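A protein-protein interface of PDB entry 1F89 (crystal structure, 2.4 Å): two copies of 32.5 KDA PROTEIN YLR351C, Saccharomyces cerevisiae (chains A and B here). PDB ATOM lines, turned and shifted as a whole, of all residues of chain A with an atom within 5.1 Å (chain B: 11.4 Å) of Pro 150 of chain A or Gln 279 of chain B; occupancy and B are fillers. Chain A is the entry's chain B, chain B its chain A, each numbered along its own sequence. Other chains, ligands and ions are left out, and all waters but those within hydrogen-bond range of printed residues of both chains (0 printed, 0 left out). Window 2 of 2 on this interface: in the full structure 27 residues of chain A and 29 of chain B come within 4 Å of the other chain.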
ATOM      1  N   TYR A 110       0.578  21.485  23.859  1.00  0.00           N
ATOM      2  CA  TYR A 110       0.417  20.094  23.458  1.00  0.00           C
ATOM      3  C   TYR A 110       1.741  19.444  23.075  1.00  0.00           C
ATOM      4  O   TYR A 110       2.790  20.078  23.095  1.00  0.00           O
ATOM      5  CB  TYR A 110      -0.514  20.016  22.242  1.00  0.00           C
ATOM      6  CG  TYR A 110      -1.924  20.503  22.479  1.00  0.00           C
ATOM      7  CD1 TYR A 110      -2.201  21.851  22.711  1.00  0.00           C
ATOM      8  CD2 TYR A 110      -2.989  19.604  22.467  1.00  0.00           C
ATOM      9  CE1 TYR A 110      -3.513  22.284  22.930  1.00  0.00           C
ATOM     10  CE2 TYR A 110      -4.291  20.024  22.683  1.00  0.00           C
ATOM     11  CZ  TYR A 110      -4.551  21.357  22.914  1.00  0.00           C
ATOM     12  OH  TYR A 110      -5.851  21.745  23.149  1.00  0.00           O
ATOM     13  N   ARG A 127      -1.726  16.073  17.385  1.00  0.00           N
ATOM     14  CA  ARG A 127      -1.587  16.395  18.799  1.00  0.00           C
ATOM     15  C   ARG A 127      -1.872  15.086  19.525  1.00  0.00           C
ATOM     16  O   ARG A 127      -2.912  14.458  19.302  1.00  0.00           O
ATOM     17  CB  ARG A 127      -2.613  17.439  19.252  1.00  0.00           C
ATOM     18  CG  ARG A 127      -2.518  18.826  18.629  1.00  0.00           C
ATOM     19  CD  ARG A 127      -3.800  19.607  18.938  1.00  0.00           C
ATOM     20  NE  ARG A 127      -3.875  20.898  18.263  1.00  0.00           N
ATOM     21  CZ  ARG A 127      -3.184  21.969  18.632  1.00  0.00           C
ATOM     22  NH1 ARG A 127      -2.365  21.899  19.672  1.00  0.00           N
ATOM     23  NH2 ARG A 127      -3.317  23.108  17.967  1.00  0.00           N
ATOM     24  N   LYS A 128      -0.944  14.676  20.381  1.00  0.00           N
ATOM     25  CA  LYS A 128      -1.090  13.448  21.150  1.00  0.00           C
ATOM     26  C   LYS A 128      -2.494  13.374  21.743  1.00  0.00           C
ATOM     27  O   LYS A 128      -2.907  14.249  22.500  1.00  0.00           O
ATOM     28  CB  LYS A 128      -0.049  13.423  22.271  1.00  0.00           C
ATOM     29  CG  LYS A 128       0.034  12.136  23.066  1.00  0.00           C
ATOM     30  CD  LYS A 128       1.118  12.271  24.121  1.00  0.00           C
ATOM     31  CE  LYS A 128       1.314  10.987  24.914  1.00  0.00           C
ATOM     32  NZ  LYS A 128       2.482  11.078  25.849  1.00  0.00           N
ATOM     33  N   VAL A 129      -3.228  12.333  21.379  1.00  0.00           N
ATOM     34  CA  VAL A 129      -4.577  12.135  21.873  1.00  0.00           C
ATOM     35  C   VAL A 129      -4.542  11.574  23.296  1.00  0.00           C
ATOM     36  O   VAL A 129      -4.777  12.294  24.263  1.00  0.00           O
ATOM     37  CB  VAL A 129      -5.352  11.165  20.962  1.00  0.00           C
ATOM     38  CG1 VAL A 129      -6.727  10.873  21.551  1.00  0.00           C
ATOM     39  CG2 VAL A 129      -5.483  11.765  19.574  1.00  0.00           C
ATOM     40  N   HIS A 130      -4.228  10.290  23.418  1.00  0.00           N
ATOM     41  CA  HIS A 130      -4.172   9.624  24.712  1.00  0.00           C
ATOM     42  C   HIS A 130      -2.925   9.973  25.527  1.00  0.00           C
ATOM     43  O   HIS A 130      -1.801   9.790  25.059  1.00  0.00           O
ATOM     44  CB  HIS A 130      -4.234   8.127  24.477  1.00  0.00           C
ATOM     45  CG  HIS A 130      -5.315   7.730  23.528  1.00  0.00           C
ATOM     46  ND1 HIS A 130      -6.601   7.451  23.937  1.00  0.00           N
ATOM     47  CD2 HIS A 130      -5.315   7.618  22.179  1.00  0.00           C
ATOM     48  CE1 HIS A 130      -7.349   7.182  22.882  1.00  0.00           C
ATOM     49  NE2 HIS A 130      -6.593   7.277  21.802  1.00  0.00           N
ATOM     50  N   LEU A 131      -3.119  10.461  26.750  1.00  0.00           N
ATOM     51  CA  LEU A 131      -1.992  10.825  27.609  1.00  0.00           C
ATOM     52  C   LEU A 131      -2.277  10.615  29.093  1.00  0.00           C
ATOM     53  O   LEU A 131      -1.521   9.930  29.788  1.00  0.00           O
ATOM     54  CB  LEU A 131      -1.598  12.278  27.346  1.00  0.00           C
ATOM     55  CG  LEU A 131      -2.728  13.306  27.394  1.00  0.00           C
ATOM     56  CD1 LEU A 131      -2.978  13.742  28.830  1.00  0.00           C
ATOM     57  CD2 LEU A 131      -2.347  14.504  26.541  1.00  0.00           C
ATOM     58  N   LEU A 148       0.124  19.108  29.984  1.00  0.00           N
ATOM     59  CA  LEU A 148      -0.255  19.061  28.585  1.00  0.00           C
ATOM     60  C   LEU A 148      -1.747  18.852  28.410  1.00  0.00           C
ATOM     61  O   LEU A 148      -2.431  18.391  29.322  1.00  0.00           O
ATOM     62  CB  LEU A 148       0.496  17.932  27.875  1.00  0.00           C
ATOM     63  CG  LEU A 148       2.016  17.949  28.015  1.00  0.00           C
ATOM     64  CD1 LEU A 148       2.601  16.774  27.261  1.00  0.00           C
ATOM     65  CD2 LEU A 148       2.570  19.261  27.491  1.00  0.00           C
ATOM     66  N   SER A 149      -2.236  19.200  27.225  1.00  0.00           N
ATOM     67  CA  SER A 149      -3.634  19.045  26.877  1.00  0.00           C
ATOM     68  C   SER A 149      -3.719  17.973  25.790  1.00  0.00           C
ATOM     69  O   SER A 149      -2.749  17.738  25.063  1.00  0.00           O
ATOM     70  CB  SER A 149      -4.201  20.374  26.376  1.00  0.00           C
ATOM     71  OG  SER A 149      -4.136  21.364  27.393  1.00  0.00           O
ATOM     72  N   PRO A 150      -4.876  17.299  25.673  1.00  0.00           N
ATOM     73  CA  PRO A 150      -5.063  16.246  24.670  1.00  0.00           C
ATOM     74  C   PRO A 150      -5.549  16.711  23.298  1.00  0.00           C
ATOM     75  O   PRO A 150      -6.151  17.778  23.171  1.00  0.00           O
ATOM     76  CB  PRO A 150      -6.066  15.326  25.348  1.00  0.00           C
ATOM     77  CG  PRO A 150      -6.963  16.313  26.029  1.00  0.00           C
ATOM     78  CD  PRO A 150      -5.986  17.299  26.643  1.00  0.00           C
ATOM     79  N   GLY A 151      -5.278  15.895  22.279  1.00  0.00           N
ATOM     80  CA  GLY A 151      -5.707  16.201  20.927  1.00  0.00           C
ATOM     81  C   GLY A 151      -7.020  15.487  20.676  1.00  0.00           C
ATOM     82  O   GLY A 151      -7.410  14.623  21.466  1.00  0.00           O
ATOM     83  N   GLU A 152      -7.707  15.821  19.587  1.00  0.00           N
ATOM     84  CA  GLU A 152      -8.991  15.188  19.306  1.00  0.00           C
ATOM     85  C   GLU A 152      -9.143  14.635  17.908  1.00  0.00           C
ATOM     86  O   GLU A 152     -10.149  14.000  17.597  1.00  0.00           O
ATOM     87  CB  GLU A 152     -10.118  16.173  19.549  1.00  0.00           C
ATOM     88  CG  GLU A 152     -10.242  16.598  20.981  1.00  0.00           C
ATOM     89  CD  GLU A 152     -11.318  17.638  21.163  1.00  0.00           C
ATOM     90  OE1 GLU A 152     -12.423  17.451  20.602  1.00  0.00           O
ATOM     91  OE2 GLU A 152     -11.061  18.635  21.870  1.00  0.00           O
ATOM     92  N   ARG B 183     -14.760  -5.319  27.131  1.00  0.00           N
ATOM     93  CA  ARG B 183     -15.364  -4.100  27.635  1.00  0.00           C
ATOM     94  C   ARG B 183     -16.722  -4.382  28.294  1.00  0.00           C
ATOM     95  O   ARG B 183     -17.226  -3.569  29.071  1.00  0.00           O
ATOM     96  CB  ARG B 183     -15.459  -3.069  26.501  1.00  0.00           C
ATOM     97  CG  ARG B 183     -14.074  -2.532  26.108  1.00  0.00           C
ATOM     98  CD  ARG B 183     -14.049  -1.724  24.811  1.00  0.00           C
ATOM     99  NE  ARG B 183     -12.677  -1.372  24.441  1.00  0.00           N
ATOM    100  CZ  ARG B 183     -12.316  -0.923  23.244  1.00  0.00           C
ATOM    101  NH1 ARG B 183     -13.226  -0.765  22.292  1.00  0.00           N
ATOM    102  NH2 ARG B 183     -11.044  -0.644  22.993  1.00  0.00           N
ATOM    103  N   PRO B 275      -4.195   2.651  32.540  1.00  0.00           N
ATOM    104  CA  PRO B 275      -5.633   2.913  32.437  1.00  0.00           C
ATOM    105  C   PRO B 275      -6.329   2.591  31.120  1.00  0.00           C
ATOM    106  O   PRO B 275      -5.784   2.762  30.029  1.00  0.00           O
ATOM    107  CB  PRO B 275      -5.749   4.391  32.813  1.00  0.00           C
ATOM    108  CG  PRO B 275      -4.398   4.948  32.466  1.00  0.00           C
ATOM    109  CD  PRO B 275      -3.479   3.866  32.966  1.00  0.00           C
ATOM    110  N   LEU B 276      -7.556   2.112  31.260  1.00  0.00           N
ATOM    111  CA  LEU B 276      -8.397   1.749  30.135  1.00  0.00           C
ATOM    112  C   LEU B 276      -9.351   2.900  29.856  1.00  0.00           C
ATOM    113  O   LEU B 276     -10.463   2.688  29.367  1.00  0.00           O
ATOM    114  CB  LEU B 276      -9.210   0.501  30.470  1.00  0.00           C
ATOM    115  CG  LEU B 276     -10.061   0.629  31.735  1.00  0.00           C
ATOM    116  CD1 LEU B 276     -11.267  -0.272  31.619  1.00  0.00           C
ATOM    117  CD2 LEU B 276      -9.235   0.279  32.967  1.00  0.00           C
ATOM    118  N   THR B 277      -8.933   4.115  30.198  1.00  0.00           N
ATOM    119  CA  THR B 277      -9.773   5.280  29.951  1.00  0.00           C
ATOM    120  C   THR B 277      -9.322   5.856  28.609  1.00  0.00           C
ATOM    121  O   THR B 277      -8.317   6.570  28.510  1.00  0.00           O
ATOM    122  CB  THR B 277      -9.641   6.327  31.075  1.00  0.00           C
ATOM    123  OG1 THR B 277      -9.842   5.691  32.347  1.00  0.00           O
ATOM    124  CG2 THR B 277     -10.694   7.412  30.905  1.00  0.00           C
ATOM    125  N   LYS B 278     -10.085   5.502  27.583  1.00  0.00           N
ATOM    126  CA  LYS B 278      -9.819   5.889  26.209  1.00  0.00           C
ATOM    127  C   LYS B 278     -10.620   7.120  25.813  1.00  0.00           C
ATOM    128  O   LYS B 278     -11.734   7.314  26.294  1.00  0.00           O
ATOM    129  CB  LYS B 278     -10.187   4.709  25.304  1.00  0.00           C
ATOM    130  CG  LYS B 278      -9.787   3.351  25.913  1.00  0.00           C
ATOM    131  CD  LYS B 278     -10.455   2.156  25.222  1.00  0.00           C
ATOM    132  CE  LYS B 278     -10.020   0.811  25.809  1.00  0.00           C
ATOM    133  NZ  LYS B 278      -8.629   0.428  25.429  1.00  0.00           N
ATOM    134  N   GLN B 279     -10.058   7.959  24.946  1.00  0.00           N
ATOM    135  CA  GLN B 279     -10.784   9.142  24.503  1.00  0.00           C
ATOM    136  C   GLN B 279     -11.722   8.658  23.410  1.00  0.00           C
ATOM    137  O   GLN B 279     -11.398   8.696  22.225  1.00  0.00           O
ATOM    138  CB  GLN B 279      -9.837  10.231  23.970  1.00  0.00           C
ATOM    139  CG  GLN B 279     -10.530  11.598  23.812  1.00  0.00           C
ATOM    140  CD  GLN B 279      -9.592  12.732  23.420  1.00  0.00           C
ATOM    141  OE1 GLN B 279      -8.706  13.123  24.184  1.00  0.00           O
ATOM    142  NE2 GLN B 279      -9.791  13.266  22.219  1.00  0.00           N
ATOM    143  N   ARG B 280     -12.890   8.192  23.839  1.00  0.00           N
ATOM    144  CA  ARG B 280     -13.893   7.655  22.937  1.00  0.00           C
ATOM    145  C   ARG B 280     -14.279   8.552  21.756  1.00  0.00           C
ATOM    146  O   ARG B 280     -15.050   8.138  20.889  1.00  0.00           O
ATOM    147  CB  ARG B 280     -15.140   7.271  23.733  1.00  0.00           C
ATOM    148  CG  ARG B 280     -16.031   6.285  23.012  1.00  0.00           C
ATOM    149  CD  ARG B 280     -15.399   4.900  22.910  1.00  0.00           C
ATOM    150  NE  ARG B 280     -16.123   4.066  21.945  1.00  0.00           N
ATOM    151  CZ  ARG B 280     -16.422   2.779  22.121  1.00  0.00           C
ATOM    152  NH1 ARG B 280     -16.064   2.157  23.235  1.00  0.00           N
ATOM    153  NH2 ARG B 280     -17.083   2.113  21.179  1.00  0.00           N
ATOM    154  N   ARG B 281     -13.754   9.773  21.711  1.00  0.00           N
ATOM    155  CA  ARG B 281     -14.064  10.663  20.596  1.00  0.00           C
ATOM    156  C   ARG B 281     -13.276  10.261  19.343  1.00  0.00           C
ATOM    157  O   ARG B 281     -12.361  10.972  18.900  1.00  0.00           O
ATOM    158  CB  ARG B 281     -13.774  12.122  20.960  1.00  0.00           C
ATOM    159  CG  ARG B 281     -14.045  13.101  19.818  1.00  0.00           C
ATOM    160  CD  ARG B 281     -15.365  12.797  19.087  1.00  0.00           C
ATOM    161  NE  ARG B 281     -15.147  12.220  17.758  1.00  0.00           N
ATOM    162  CZ  ARG B 281     -16.118  11.843  16.929  1.00  0.00           C
ATOM    163  NH1 ARG B 281     -17.387  11.973  17.286  1.00  0.00           N
ATOM    164  NH2 ARG B 281     -15.822  11.343  15.733  1.00  0.00           N
ATOM    165  N   PHE B 282     -13.644   9.099  18.802  1.00  0.00           N
ATOM    166  CA  PHE B 282     -13.052   8.525  17.596  1.00  0.00           C
ATOM    167  C   PHE B 282     -13.729   7.212  17.261  1.00  0.00           C
ATOM    168  O   PHE B 282     -13.861   6.850  16.103  1.00  0.00           O
ATOM    169  CB  PHE B 282     -11.532   8.325  17.756  1.00  0.00           C
ATOM    170  CG  PHE B 282     -11.121   7.337  18.829  1.00  0.00           C
ATOM    171  CD1 PHE B 282     -10.070   7.646  19.689  1.00  0.00           C
ATOM    172  CD2 PHE B 282     -11.734   6.092  18.953  1.00  0.00           C
ATOM    173  CE1 PHE B 282      -9.636   6.741  20.654  1.00  0.00           C
ATOM    174  CE2 PHE B 282     -11.303   5.180  19.921  1.00  0.00           C
ATOM    175  CZ  PHE B 282     -10.248   5.508  20.772  1.00  0.00           C
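O of Gly 151 of chain A is in hydrogen-bond range of NE2 of Gln 279 of chain B, 2.8 Å away.
The backbone NH of Gly 151 of chain A sits at hydrogen-bond distance from the backbone carbonyl oxygen of Lys 128 of chain A, at 2.9 Å.
Gln 279 of chain B touches Val 129 of chain A (CD to CG1, 3.9 Å).
His 130 of chain A touches Gln 279 of chain B (CE1 to N, 3.5 Å).
Phe 282 of chain B touches His 130 of chain A.
Pro 150 of chain A touches Gln 279 of chain B (CB to OE1, 3.6 Å).
Gln 279 of chain B touches Glu 152 of chain A.
O of Glu 152 of chain A touches O of Arg 281 of chain B, 3.97 Å away.
No position is printed for both chains.
Of the 7 pairs that touch across the chains among the printed residues, none has its exchanged pair printed and touching as well.
Val 129 of chain A touches just one residue of chain B: Gln 279 (3.9 Å).
His 130 of chain A touches just these residues of chain B: Gln 279 (3.5 Å) and Phe 282 (3.2 Å).
Leu 148 of chain A touches none of the printed residues of chain B.
No residue of chain B comes within 4 Å of Ser 149 of chain A.
Of chain B, only Gln 279 comes within 4 Å of Pro 150 of chain A.
Gly 151 of chain A touches just one residue of chain B: Gln 279.
Of chain B, only Gln 279 (3.6 Å) and Arg 281 (3.97 Å) come within 4 Å of Glu 152 of chain A.
Of the printed residues of chain A, Gln 279 of chain B touches Val 129, His 130, Pro 150, Gly 151 and Glu 152.
Printed residues of chain A within 4 Å of Arg 281 of chain B: Glu 152.
Printed residues of chain A within 4 Å of Phe 282 of chain B: His 130 (3.2 Å).
The nearest printed residue of chain A that does not touch Gln 279 of chain B is Lys 128 of chain A (6.1 Å).
The nearest printed residue of chain A that does not touch Phe 282 of chain B is Val 129 of chain A (5.0 Å).
Of the 11 printed residues of chain A, 5 touch a printed residue of chain B.
Hydrophobic or aromatic side chains of chain A within 4 Å of the printed part of chain B: Val 129, His 130 and Pro 150.
Printed residues of chain B that touch a printed residue of chain A: Gln 279, Arg 281 and Phe 282.
Hydrophobic or aromatic side chains of chain B that line the printed part of chain A: Phe 282.
Among the printed residues, 7 pairs touch across the chains.
Among the printed residues, no Asp or Glu carboxylate lies within 4 Å of a Lys or Arg side-chain nitrogen of the other chain.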
